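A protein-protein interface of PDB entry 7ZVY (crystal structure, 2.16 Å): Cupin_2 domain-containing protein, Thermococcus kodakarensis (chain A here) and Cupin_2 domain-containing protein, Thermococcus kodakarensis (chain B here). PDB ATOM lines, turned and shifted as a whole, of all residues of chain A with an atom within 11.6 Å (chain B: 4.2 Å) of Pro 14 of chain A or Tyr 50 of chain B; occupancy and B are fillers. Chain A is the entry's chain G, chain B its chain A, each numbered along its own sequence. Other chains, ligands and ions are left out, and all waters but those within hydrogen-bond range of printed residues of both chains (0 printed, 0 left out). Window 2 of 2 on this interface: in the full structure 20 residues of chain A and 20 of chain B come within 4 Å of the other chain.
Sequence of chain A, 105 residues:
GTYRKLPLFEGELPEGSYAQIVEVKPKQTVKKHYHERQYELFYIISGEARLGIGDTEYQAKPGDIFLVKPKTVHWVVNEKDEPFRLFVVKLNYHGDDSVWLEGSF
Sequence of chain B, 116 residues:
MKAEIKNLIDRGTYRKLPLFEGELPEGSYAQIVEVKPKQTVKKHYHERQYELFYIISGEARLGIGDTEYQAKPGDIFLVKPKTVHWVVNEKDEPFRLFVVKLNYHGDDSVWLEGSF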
ATOM      1  N   LEU A   8     -24.990   9.411   9.714  1.00  0.00           N
ATOM      2  CA  LEU A   8     -25.485   8.104   9.215  1.00  0.00           C
ATOM      3  C   LEU A   8     -24.815   7.827   7.874  1.00  0.00           C
ATOM      4  O   LEU A   8     -24.357   8.776   7.279  1.00  0.00           O
ATOM      5  CB  LEU A   8     -26.992   8.164   8.969  1.00  0.00           C
ATOM      6  CG  LEU A   8     -27.959   8.385  10.128  1.00  0.00           C
ATOM      7  CD1 LEU A   8     -27.280   8.315  11.502  1.00  0.00           C
ATOM      8  CD2 LEU A   8     -28.717   9.686   9.941  1.00  0.00           C
ATOM      9  N   PHE A   9     -24.782   6.571   7.416  1.00  0.00           N
ATOM     10  CA  PHE A   9     -24.563   6.231   5.988  1.00  0.00           C
ATOM     11  C   PHE A   9     -23.302   6.967   5.514  1.00  0.00           C
ATOM     12  O   PHE A   9     -23.261   7.526   4.393  1.00  0.00           O
ATOM     13  CB  PHE A   9     -25.839   6.558   5.199  1.00  0.00           C
ATOM     14  CG  PHE A   9     -27.068   5.806   5.661  1.00  0.00           C
ATOM     15  CD1 PHE A   9     -27.155   5.238   6.931  1.00  0.00           C
ATOM     16  CD2 PHE A   9     -28.166   5.684   4.824  1.00  0.00           C
ATOM     17  CE1 PHE A   9     -28.291   4.550   7.339  1.00  0.00           C
ATOM     18  CE2 PHE A   9     -29.313   5.025   5.244  1.00  0.00           C
ATOM     19  CZ  PHE A   9     -29.370   4.441   6.493  1.00  0.00           C
ATOM     20  N   GLU A  10     -22.289   6.869   6.372  1.00  0.00           N
ATOM     21  CA  GLU A  10     -20.912   7.417   6.196  1.00  0.00           C
ATOM     22  C   GLU A  10     -20.192   6.673   5.061  1.00  0.00           C
ATOM     23  O   GLU A  10     -20.085   5.431   5.141  1.00  0.00           O
ATOM     24  CB  GLU A  10     -20.156   7.260   7.518  1.00  0.00           C
ATOM     25  CG  GLU A  10     -21.092   7.225   8.719  1.00  0.00           C
ATOM     26  CD  GLU A  10     -20.417   7.089  10.072  1.00  0.00           C
ATOM     27  OE1 GLU A  10     -21.066   6.547  11.003  1.00  0.00           O
ATOM     28  OE2 GLU A  10     -19.251   7.506  10.185  1.00  0.00           O
ATOM     29  N   GLY A  11     -19.721   7.403   4.042  1.00  0.00           N
ATOM     30  CA  GLY A  11     -19.034   6.838   2.865  1.00  0.00           C
ATOM     31  C   GLY A  11     -19.987   6.233   1.841  1.00  0.00           C
ATOM     32  O   GLY A  11     -19.512   5.888   0.682  1.00  0.00           O
ATOM     33  N   GLU A  12     -21.253   6.093   2.241  1.00  0.00           N
ATOM     34  CA  GLU A  12     -22.350   5.495   1.444  1.00  0.00           C
ATOM     35  C   GLU A  12     -23.036   6.579   0.617  1.00  0.00           C
ATOM     36  O   GLU A  12     -23.528   6.242  -0.479  1.00  0.00           O
ATOM     37  CB  GLU A  12     -23.361   4.802   2.364  1.00  0.00           C
ATOM     38  CG  GLU A  12     -22.831   3.522   2.980  1.00  0.00           C
ATOM     39  CD  GLU A  12     -22.398   2.493   1.949  1.00  0.00           C
ATOM     40  OE1 GLU A  12     -22.772   2.657   0.740  1.00  0.00           O
ATOM     41  OE2 GLU A  12     -21.666   1.550   2.339  1.00  0.00           O
ATOM     42  N   LEU A  13     -23.048   7.823   1.114  1.00  0.00           N
ATOM     43  CA  LEU A  13     -23.735   8.954   0.445  1.00  0.00           C
ATOM     44  C   LEU A  13     -22.850   9.531  -0.650  1.00  0.00           C
ATOM     45  O   LEU A  13     -21.662   9.792  -0.431  1.00  0.00           O
ATOM     46  CB  LEU A  13     -24.108  10.028   1.467  1.00  0.00           C
ATOM     47  CG  LEU A  13     -25.140   9.587   2.497  1.00  0.00           C
ATOM     48  CD1 LEU A  13     -25.407  10.697   3.503  1.00  0.00           C
ATOM     49  CD2 LEU A  13     -26.439   9.167   1.810  1.00  0.00           C
ATOM     50  N   PRO A  14     -23.445   9.738  -1.853  1.00  0.00           N
ATOM     51  CA  PRO A  14     -22.732  10.292  -3.007  1.00  0.00           C
ATOM     52  C   PRO A  14     -21.862  11.516  -2.687  1.00  0.00           C
ATOM     53  O   PRO A  14     -21.874  11.969  -1.541  1.00  0.00           O
ATOM     54  CB  PRO A  14     -23.838  10.721  -3.987  1.00  0.00           C
ATOM     55  CG  PRO A  14     -25.138  10.112  -3.460  1.00  0.00           C
ATOM     56  CD  PRO A  14     -24.843   9.348  -2.174  1.00  0.00           C
ATOM     57  N   GLU A  15     -21.126  11.991  -3.704  1.00  0.00           N
ATOM     58  CA  GLU A  15     -20.179  13.138  -3.629  1.00  0.00           C
ATOM     59  C   GLU A  15     -20.960  14.392  -3.241  1.00  0.00           C
ATOM     60  O   GLU A  15     -21.949  14.724  -3.941  1.00  0.00           O
ATOM     61  CB  GLU A  15     -19.472  13.371  -4.970  1.00  0.00           C
ATOM     62  CG  GLU A  15     -18.611  14.640  -5.018  1.00  0.00           C
ATOM     63  CD  GLU A  15     -17.320  14.561  -5.830  1.00  0.00           C
ATOM     64  OE1 GLU A  15     -17.119  13.551  -6.546  1.00  0.00           O
ATOM     65  OE2 GLU A  15     -16.519  15.536  -5.761  1.00  0.00           O
ATOM     66  N   GLY A  16     -20.536  15.048  -2.161  1.00  0.00           N
ATOM     67  CA  GLY A  16     -21.130  16.323  -1.741  1.00  0.00           C
ATOM     68  C   GLY A  16     -22.387  16.110  -0.935  1.00  0.00           C
ATOM     69  O   GLY A  16     -22.865  17.106  -0.376  1.00  0.00           O
ATOM     70  N   SER A  17     -22.887  14.872  -0.844  1.00  0.00           N
ATOM     71  CA  SER A  17     -24.083  14.570  -0.026  1.00  0.00           C
ATOM     72  C   SER A  17     -23.645  14.309   1.401  1.00  0.00           C
ATOM     73  O   SER A  17     -22.473  13.933   1.618  1.00  0.00           O
ATOM     74  CB  SER A  17     -24.878  13.403  -0.537  1.00  0.00           C
ATOM     75  OG  SER A  17     -25.849  13.860  -1.478  1.00  0.00           O
ATOM     76  N   TYR A  18     -24.585  14.440   2.330  1.00  0.00           N
ATOM     77  CA  TYR A  18     -24.298  14.149   3.740  1.00  0.00           C
ATOM     78  C   TYR A  18     -25.598  14.040   4.502  1.00  0.00           C
ATOM     79  O   TYR A  18     -26.537  14.780   4.200  1.00  0.00           O
ATOM     80  CB  TYR A  18     -23.428  15.253   4.322  1.00  0.00           C
ATOM     81  CG  TYR A  18     -22.689  14.793   5.540  1.00  0.00           C
ATOM     82  CD1 TYR A  18     -21.650  13.885   5.422  1.00  0.00           C
ATOM     83  CD2 TYR A  18     -23.088  15.186   6.807  1.00  0.00           C
ATOM     84  CE1 TYR A  18     -20.947  13.468   6.536  1.00  0.00           C
ATOM     85  CE2 TYR A  18     -22.409  14.754   7.933  1.00  0.00           C
ATOM     86  CZ  TYR A  18     -21.354  13.872   7.795  1.00  0.00           C
ATOM     87  OH  TYR A  18     -20.655  13.422   8.873  1.00  0.00           O
ATOM     88  N   ALA A  19     -25.645  13.146   5.484  1.00  0.00           N
ATOM     89  CA  ALA A  19     -26.871  12.974   6.295  1.00  0.00           C
ATOM     90  C   ALA A  19     -26.500  12.653   7.729  1.00  0.00           C
ATOM     91  O   ALA A  19     -25.528  11.998   7.946  1.00  0.00           O
ATOM     92  CB  ALA A  19     -27.714  11.885   5.705  1.00  0.00           C
ATOM     93  N   LEU A  41     -31.044  20.593   4.946  1.00  0.00           N
ATOM     94  CA  LEU A  41     -32.486  20.193   5.051  1.00  0.00           C
ATOM     95  C   LEU A  41     -32.793  19.650   6.430  1.00  0.00           C
ATOM     96  O   LEU A  41     -32.277  18.624   6.731  1.00  0.00           O
ATOM     97  CB  LEU A  41     -32.833  19.119   4.024  1.00  0.00           C
ATOM     98  CG  LEU A  41     -33.536  19.660   2.790  1.00  0.00           C
ATOM     99  CD1 LEU A  41     -33.576  18.606   1.692  1.00  0.00           C
ATOM    100  CD2 LEU A  41     -34.918  20.073   3.160  1.00  0.00           C
ATOM    101  N   PHE A  87     -33.454  15.778  11.819  1.00  0.00           N
ATOM    102  CA  PHE A  87     -32.847  14.904  10.794  1.00  0.00           C
ATOM    103  C   PHE A  87     -32.225  15.898   9.837  1.00  0.00           C
ATOM    104  O   PHE A  87     -32.906  16.817   9.354  1.00  0.00           O
ATOM    105  CB  PHE A  87     -33.864  13.917  10.177  1.00  0.00           C
ATOM    106  CG  PHE A  87     -33.282  13.205   8.987  1.00  0.00           C
ATOM    107  CD1 PHE A  87     -32.190  12.372   9.132  1.00  0.00           C
ATOM    108  CD2 PHE A  87     -33.844  13.356   7.722  1.00  0.00           C
ATOM    109  CE1 PHE A  87     -31.649  11.726   8.031  1.00  0.00           C
ATOM    110  CE2 PHE A  87     -33.275  12.733   6.628  1.00  0.00           C
ATOM    111  CZ  PHE A  87     -32.170  11.943   6.783  1.00  0.00           C
ATOM    112  N   VAL A  89     -30.066  16.852   6.330  1.00  0.00           N
ATOM    113  CA  VAL A  89     -29.360  16.438   5.092  1.00  0.00           C
ATOM    114  C   VAL A  89     -28.607  17.660   4.550  1.00  0.00           C
ATOM    115  O   VAL A  89     -29.063  18.808   4.625  1.00  0.00           O
ATOM    116  CB  VAL A  89     -30.306  15.734   4.104  1.00  0.00           C
ATOM    117  CG1 VAL A  89     -29.496  15.069   3.006  1.00  0.00           C
ATOM    118  CG2 VAL A  89     -31.166  14.722   4.831  1.00  0.00           C
ATOM    119  N   LYS A  90     -27.396  17.434   4.079  1.00  0.00           N
ATOM    120  CA  LYS A  90     -26.625  18.593   3.611  1.00  0.00           C
ATOM    121  C   LYS A  90     -26.390  18.414   2.125  1.00  0.00           C
ATOM    122  O   LYS A  90     -25.921  17.354   1.691  1.00  0.00           O
ATOM    123  CB  LYS A  90     -25.362  18.779   4.460  1.00  0.00           C
ATOM    124  CG  LYS A  90     -25.681  18.914   5.945  1.00  0.00           C
ATOM    125  CD  LYS A  90     -24.436  19.072   6.831  1.00  0.00           C
ATOM    126  CE  LYS A  90     -24.808  19.307   8.284  1.00  0.00           C
ATOM    127  NZ  LYS A  90     -25.381  20.661   8.528  1.00  0.00           N
ATOM    128  N   LEU A  91     -26.729  19.444   1.365  1.00  0.00           N
ATOM    129  CA  LEU A  91     -26.587  19.377  -0.095  1.00  0.00           C
ATOM    130  C   LEU A  91     -25.530  20.370  -0.540  1.00  0.00           C
ATOM    131  O   LEU A  91     -25.262  21.385   0.191  1.00  0.00           O
ATOM    132  CB  LEU A  91     -27.929  19.667  -0.756  1.00  0.00           C
ATOM    133  CG  LEU A  91     -29.091  18.780  -0.317  1.00  0.00           C
ATOM    134  CD1 LEU A  91     -30.326  19.204  -1.077  1.00  0.00           C
ATOM    135  CD2 LEU A  91     -28.801  17.296  -0.570  1.00  0.00           C
ATOM    136  N   ASN A  92     -25.003  20.100  -1.726  1.00  0.00           N
ATOM    137  CA  ASN A  92     -23.760  20.750  -2.205  1.00  0.00           C
ATOM    138  C   ASN A  92     -22.881  20.975  -0.965  1.00  0.00           C
ATOM    139  O   ASN A  92     -22.816  22.132  -0.482  1.00  0.00           O
ATOM    140  CB  ASN A  92     -24.096  22.032  -2.967  1.00  0.00           C
ATOM    141  CG  ASN A  92     -23.076  22.353  -4.034  1.00  0.00           C
ATOM    142  OD1 ASN A  92     -22.173  23.162  -3.804  1.00  0.00           O
ATOM    143  ND2 ASN A  92     -23.190  21.702  -5.186  1.00  0.00           N
ATOM    144  N   TYR A  93     -22.345  19.881  -0.400  1.00  0.00           N
ATOM    145  CA  TYR A  93     -21.520  19.874   0.836  1.00  0.00           C
ATOM    146  C   TYR A  93     -20.062  19.654   0.420  1.00  0.00           C
ATOM    147  O   TYR A  93     -19.750  18.556  -0.083  1.00  0.00           O
ATOM    148  CB  TYR A  93     -22.075  18.783   1.763  1.00  0.00           C
ATOM    149  CG  TYR A  93     -21.249  18.353   2.952  1.00  0.00           C
ATOM    150  CD1 TYR A  93     -21.457  18.913   4.211  1.00  0.00           C
ATOM    151  CD2 TYR A  93     -20.327  17.317   2.843  1.00  0.00           C
ATOM    152  CE1 TYR A  93     -20.723  18.496   5.315  1.00  0.00           C
ATOM    153  CE2 TYR A  93     -19.625  16.852   3.948  1.00  0.00           C
ATOM    154  CZ  TYR A  93     -19.809  17.455   5.187  1.00  0.00           C
ATOM    155  OH  TYR A  93     -19.092  17.029   6.278  1.00  0.00           O
ATOM    156  N   HIS A  94     -19.218  20.686   0.557  1.00  0.00           N
ATOM    157  CA  HIS A  94     -17.756  20.620   0.283  1.00  0.00           C
ATOM    158  C   HIS A  94     -16.990  20.524   1.610  1.00  0.00           C
ATOM    159  O   HIS A  94     -15.903  21.117   1.694  1.00  0.00           O
ATOM    160  CB  HIS A  94     -17.281  21.832  -0.536  1.00  0.00           C
ATOM    161  CG  HIS A  94     -18.069  22.101  -1.778  1.00  0.00           C
ATOM    162  ND1 HIS A  94     -17.626  21.724  -3.041  1.00  0.00           N
ATOM    163  CD2 HIS A  94     -19.285  22.692  -1.950  1.00  0.00           C
ATOM    164  CE1 HIS A  94     -18.522  22.090  -3.936  1.00  0.00           C
ATOM    165  NE2 HIS A  94     -19.540  22.709  -3.294  1.00  0.00           N
ATOM    166  N   GLY A  95     -17.554  19.844   2.618  1.00  0.00           N
ATOM    167  CA  GLY A  95     -16.936  19.692   3.948  1.00  0.00           C
ATOM    168  C   GLY A  95     -17.379  20.786   4.894  1.00  0.00           C
ATOM    169  O   GLY A  95     -18.552  21.207   4.817  1.00  0.00           O
ATOM    170  N   ARG B  48     -29.640   6.114 -11.156  1.00  0.00           N
ATOM    171  CA  ARG B  48     -28.526   6.471 -10.229  1.00  0.00           C
ATOM    172  C   ARG B  48     -28.956   7.263  -9.005  1.00  0.00           C
ATOM    173  O   ARG B  48     -28.004   7.652  -8.167  1.00  0.00           O
ATOM    174  CB  ARG B  48     -27.514   7.502 -10.697  1.00  0.00           C
ATOM    175  CG  ARG B  48     -27.002   7.544 -12.106  1.00  0.00           C
ATOM    176  CD  ARG B  48     -26.237   8.835 -11.768  1.00  0.00           C
ATOM    177  NE  ARG B  48     -25.848   9.361 -13.033  1.00  0.00           N
ATOM    178  CZ  ARG B  48     -26.542  10.173 -13.802  1.00  0.00           C
ATOM    179  NH1 ARG B  48     -26.069  10.386 -15.019  1.00  0.00           N
ATOM    180  NH2 ARG B  48     -27.548  10.912 -13.345  1.00  0.00           N
ATOM    181  N   GLN B  49     -30.271   7.631  -8.906  1.00  0.00           N
ATOM    182  CA  GLN B  49     -30.514   8.574  -7.777  1.00  0.00           C
ATOM    183  C   GLN B  49     -30.492   7.774  -6.490  1.00  0.00           C
ATOM    184  O   GLN B  49     -30.801   6.547  -6.504  1.00  0.00           O
ATOM    185  CB  GLN B  49     -31.807   9.360  -7.939  1.00  0.00           C
ATOM    186  CG  GLN B  49     -32.968   8.661  -7.269  1.00  0.00           C
ATOM    187  CD  GLN B  49     -34.296   8.962  -7.907  1.00  0.00           C
ATOM    188  OE1 GLN B  49     -35.355   8.537  -7.452  1.00  0.00           O
ATOM    189  NE2 GLN B  49     -34.238   9.727  -8.992  1.00  0.00           N
ATOM    190  N   TYR B  50     -30.090   8.431  -5.423  1.00  0.00           N
ATOM    191  CA  TYR B  50     -30.187   7.831  -4.079  1.00  0.00           C
ATOM    192  C   TYR B  50     -31.450   8.368  -3.445  1.00  0.00           C
ATOM    193  O   TYR B  50     -31.837   9.482  -3.761  1.00  0.00           O
ATOM    194  CB  TYR B  50     -28.980   8.141  -3.204  1.00  0.00           C
ATOM    195  CG  TYR B  50     -27.684   7.523  -3.665  1.00  0.00           C
ATOM    196  CD1 TYR B  50     -26.916   6.767  -2.789  1.00  0.00           C
ATOM    197  CD2 TYR B  50     -27.182   7.759  -4.926  1.00  0.00           C
ATOM    198  CE1 TYR B  50     -25.696   6.230  -3.159  1.00  0.00           C
ATOM    199  CE2 TYR B  50     -25.970   7.222  -5.319  1.00  0.00           C
ATOM    200  CZ  TYR B  50     -25.227   6.452  -4.441  1.00  0.00           C
ATOM    201  OH  TYR B  50     -24.034   5.915  -4.837  1.00  0.00           O
ATOM    202  N   GLU B  51     -32.059   7.568  -2.583  1.00  0.00           N
ATOM    203  CA  GLU B  51     -33.289   7.980  -1.888  1.00  0.00           C
ATOM    204  C   GLU B  51     -33.033   7.831  -0.407  1.00  0.00           C
ATOM    205  O   GLU B  51     -32.911   6.661   0.054  1.00  0.00           O
ATOM    206  CB  GLU B  51     -34.472   7.143  -2.373  1.00  0.00           C
ATOM    207  CG  GLU B  51     -35.126   7.688  -3.637  1.00  0.00           C
ATOM    208  CD  GLU B  51     -36.487   7.061  -3.924  1.00  0.00           C
ATOM    209  OE1 GLU B  51     -36.780   6.031  -3.270  1.00  0.00           O
ATOM    210  OE2 GLU B  51     -37.248   7.571  -4.829  1.00  0.00           O
ATOM    211  N   LEU B  52     -32.997   8.962   0.314  1.00  0.00           N
ATOM    212  CA  LEU B  52     -32.996   8.908   1.788  1.00  0.00           C
ATOM    213  C   LEU B  52     -34.424   9.020   2.255  1.00  0.00           C
ATOM    214  O   LEU B  52     -35.006   9.998   1.879  1.00  0.00           O
ATOM    215  CB  LEU B  52     -32.227  10.099   2.342  1.00  0.00           C
ATOM    216  CG  LEU B  52     -30.749   9.812   2.415  1.00  0.00           C
ATOM    217  CD1 LEU B  52     -29.977  11.085   2.658  1.00  0.00           C
ATOM    218  CD2 LEU B  52     -30.482   8.729   3.452  1.00  0.00           C
ATOM    219  N   LEU B  78     -31.710   4.237   3.257  1.00  0.00           N
ATOM    220  CA  LEU B  78     -31.091   4.692   1.986  1.00  0.00           C
ATOM    221  C   LEU B  78     -31.356   3.595   0.965  1.00  0.00           C
ATOM    222  O   LEU B  78     -31.297   2.398   1.339  1.00  0.00           O
ATOM    223  CB  LEU B  78     -29.596   4.937   2.213  1.00  0.00           C
ATOM    224  CG  LEU B  78     -28.672   4.928   1.005  1.00  0.00           C
ATOM    225  CD1 LEU B  78     -28.811   6.223   0.213  1.00  0.00           C
ATOM    226  CD2 LEU B  78     -27.243   4.741   1.483  1.00  0.00           C
ATOM    227  N   VAL B  79     -31.673   3.979  -0.267  1.00  0.00           N
ATOM    228  CA  VAL B  79     -31.833   2.990  -1.379  1.00  0.00           C
ATOM    229  C   VAL B  79     -30.788   3.297  -2.454  1.00  0.00           C
ATOM    230  O   VAL B  79     -31.100   4.138  -3.383  1.00  0.00           O
ATOM    231  CB  VAL B  79     -33.241   2.984  -1.996  1.00  0.00           C
ATOM    232  CG1 VAL B  79     -33.306   1.885  -3.040  1.00  0.00           C
ATOM    233  CG2 VAL B  79     -34.310   2.814  -0.925  1.00  0.00           C
ATOM    234  N   LYS B  80     -29.573   2.766  -2.293  1.00  0.00           N
ATOM    235  CA  LYS B  80     -28.424   3.160  -3.167  1.00  0.00           C
ATOM    236  C   LYS B  80     -28.911   2.826  -4.579  1.00  0.00           C
ATOM    237  O   LYS B  80     -29.961   2.165  -4.767  1.00  0.00           O
ATOM    238  CB  LYS B  80     -27.124   2.542  -2.627  1.00  0.00           C
ATOM    239  CG  LYS B  80     -26.730   2.904  -1.193  1.00  0.00           C
ATOM    240  CD  LYS B  80     -27.197   1.875  -0.147  1.00  0.00           C
ATOM    241  CE  LYS B  80     -26.212   1.634   0.991  1.00  0.00           C
ATOM    242  NZ  LYS B  80     -26.868   0.998   2.156  1.00  0.00           N
ATOM    243  N   PRO B  81     -28.295   3.366  -5.645  1.00  0.00           N
ATOM    244  CA  PRO B  81     -28.859   3.163  -6.972  1.00  0.00           C
ATOM    245  C   PRO B  81     -28.608   1.700  -7.361  1.00  0.00           C
ATOM    246  O   PRO B  81     -27.685   1.076  -6.828  1.00  0.00           O
ATOM    247  CB  PRO B  81     -28.127   4.166  -7.864  1.00  0.00           C
ATOM    248  CG  PRO B  81     -26.917   4.624  -7.073  1.00  0.00           C
ATOM    249  CD  PRO B  81     -26.994   4.041  -5.679  1.00  0.00           C
ATOM    250  N   VAL B 100     -35.548  12.477   0.473  1.00  0.00           N
ATOM    251  CA  VAL B 100     -34.682  13.319  -0.398  1.00  0.00           C
ATOM    252  C   VAL B 100     -34.064  12.413  -1.441  1.00  0.00           C
ATOM    253  O   VAL B 100     -33.696  11.316  -1.091  1.00  0.00           O
ATOM    254  CB  VAL B 100     -33.621  14.007   0.456  1.00  0.00           C
ATOM    255  CG1 VAL B 100     -32.832  15.011  -0.369  1.00  0.00           C
ATOM    256  CG2 VAL B 100     -34.305  14.642   1.690  1.00  0.00           C
ATOM    257  N   LYS B 101     -33.910  12.916  -2.670  1.00  0.00           N
ATOM    258  CA  LYS B 101     -33.243  12.138  -3.747  1.00  0.00           C
ATOM    259  C   LYS B 101     -31.842  12.716  -3.974  1.00  0.00           C
ATOM    260  O   LYS B 101     -31.726  13.955  -4.058  1.00  0.00           O
ATOM    261  CB  LYS B 101     -34.077  12.182  -5.029  1.00  0.00           C
ATOM    262  CG  LYS B 101     -35.536  12.568  -4.832  1.00  0.00           C
ATOM    263  CD  LYS B 101     -36.384  12.313  -6.054  1.00  0.00           C
ATOM    264  CE  LYS B 101     -37.774  11.816  -5.722  1.00  0.00           C
ATOM    265  NZ  LYS B 101     -38.771  12.291  -6.709  1.00  0.00           N
ATOM    266  N   LEU B 102     -30.825  11.853  -4.069  1.00  0.00           N
ATOM    267  CA  LEU B 102     -29.421  12.314  -4.242  1.00  0.00           C
ATOM    268  C   LEU B 102     -28.897  11.796  -5.584  1.00  0.00           C
ATOM    269  O   LEU B 102     -29.109  10.606  -5.857  1.00  0.00           O
ATOM    270  CB  LEU B 102     -28.574  11.785  -3.080  1.00  0.00           C
ATOM    271  CG  LEU B 102     -29.337  11.494  -1.788  1.00  0.00           C
ATOM    272  CD1 LEU B 102     -28.481  10.683  -0.829  1.00  0.00           C
ATOM    273  CD2 LEU B 102     -29.799  12.783  -1.125  1.00  0.00           C
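The backbone NH of Leu 52 of chain B lies within hydrogen-bond range of the backbone carbonyl oxygen of Val 100 of chain B (2.8 Å). The backbone NH (N) of Leu 8 of chain A lies within hydrogen-bond range of the backbone carbonyl oxygen (O) of Ala 19 of chain A (3.2 Å). The backbone NH of Tyr 50 of chain B sits at hydrogen-bond distance from the backbone carbonyl oxygen of Leu 102 of chain B (2.4 Å).
Leu 78 of chain B touches Phe 9 of chain A. CE1 of Tyr 50 of chain B touches O of Glu 12 of chain A, 3.4 Å away. Leu 78 of chain B touches Glu 12 of chain A (CD2 to CB, 3.98 Å). Lys 80 of chain B touches Glu 12 of chain A (CE to OE1, 3.6 Å). Leu 13 of chain A touches Leu 102 of chain B. Tyr 50 of chain B touches Pro 14 of chain A (CD1 to CD, 3.4 Å). CG of Pro 14 of chain A touches CB of Leu 102 of chain B, 3.8 Å away. Ser 17 of chain A touches Leu 102 of chain B. Ala 19 of chain A touches Leu 52 of chain B.
Of the printed residues of chain B, Phe 9 of chain A touches Leu 78 (3.0 Å). Of the printed residues of chain B, Glu 12 of chain A touches Tyr 50 (3.4 Å), Leu 78 (3.98 Å) and Lys 80 (3.6 Å). Pro 14 of chain A touches just these residues of chain B: Tyr 50 and Leu 102. Of the printed residues of chain B, Ser 17 of chain A touches Leu 102. Printed residues of chain B within 4 Å of Ala 19 of chain A: Leu 52. No residue of chain A comes within 4 Å of Gln 49 of chain B. Tyr 50 of chain B touches two residues of chain A. No residue of chain A comes within 4 Å of Glu 51 of chain B. No residue of chain A comes within 4 Å of Pro 81 of chain B. Leu 102 of chain B touches three residues of chain A. The nearest printed residue of chain B that does not touch Ser 17 of chain A is Lys 101 of chain B (6.4 Å).
Of the 12 printed residues of chain B, 5 touch a printed residue of chain A. Hydrophobic or aromatic side chains of chain B that line the printed part of chain A: Tyr 50, Leu 52, Leu 78 and Leu 102. Of the 21 printed residues of chain A, 6 touch a printed residue of chain B. Hydrophobic or aromatic side chains of chain A that line the printed part of chain B: Phe 9, Leu 13, Pro 14 and Ala 19. Among the printed residues, 9 pairs touch across the chains.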
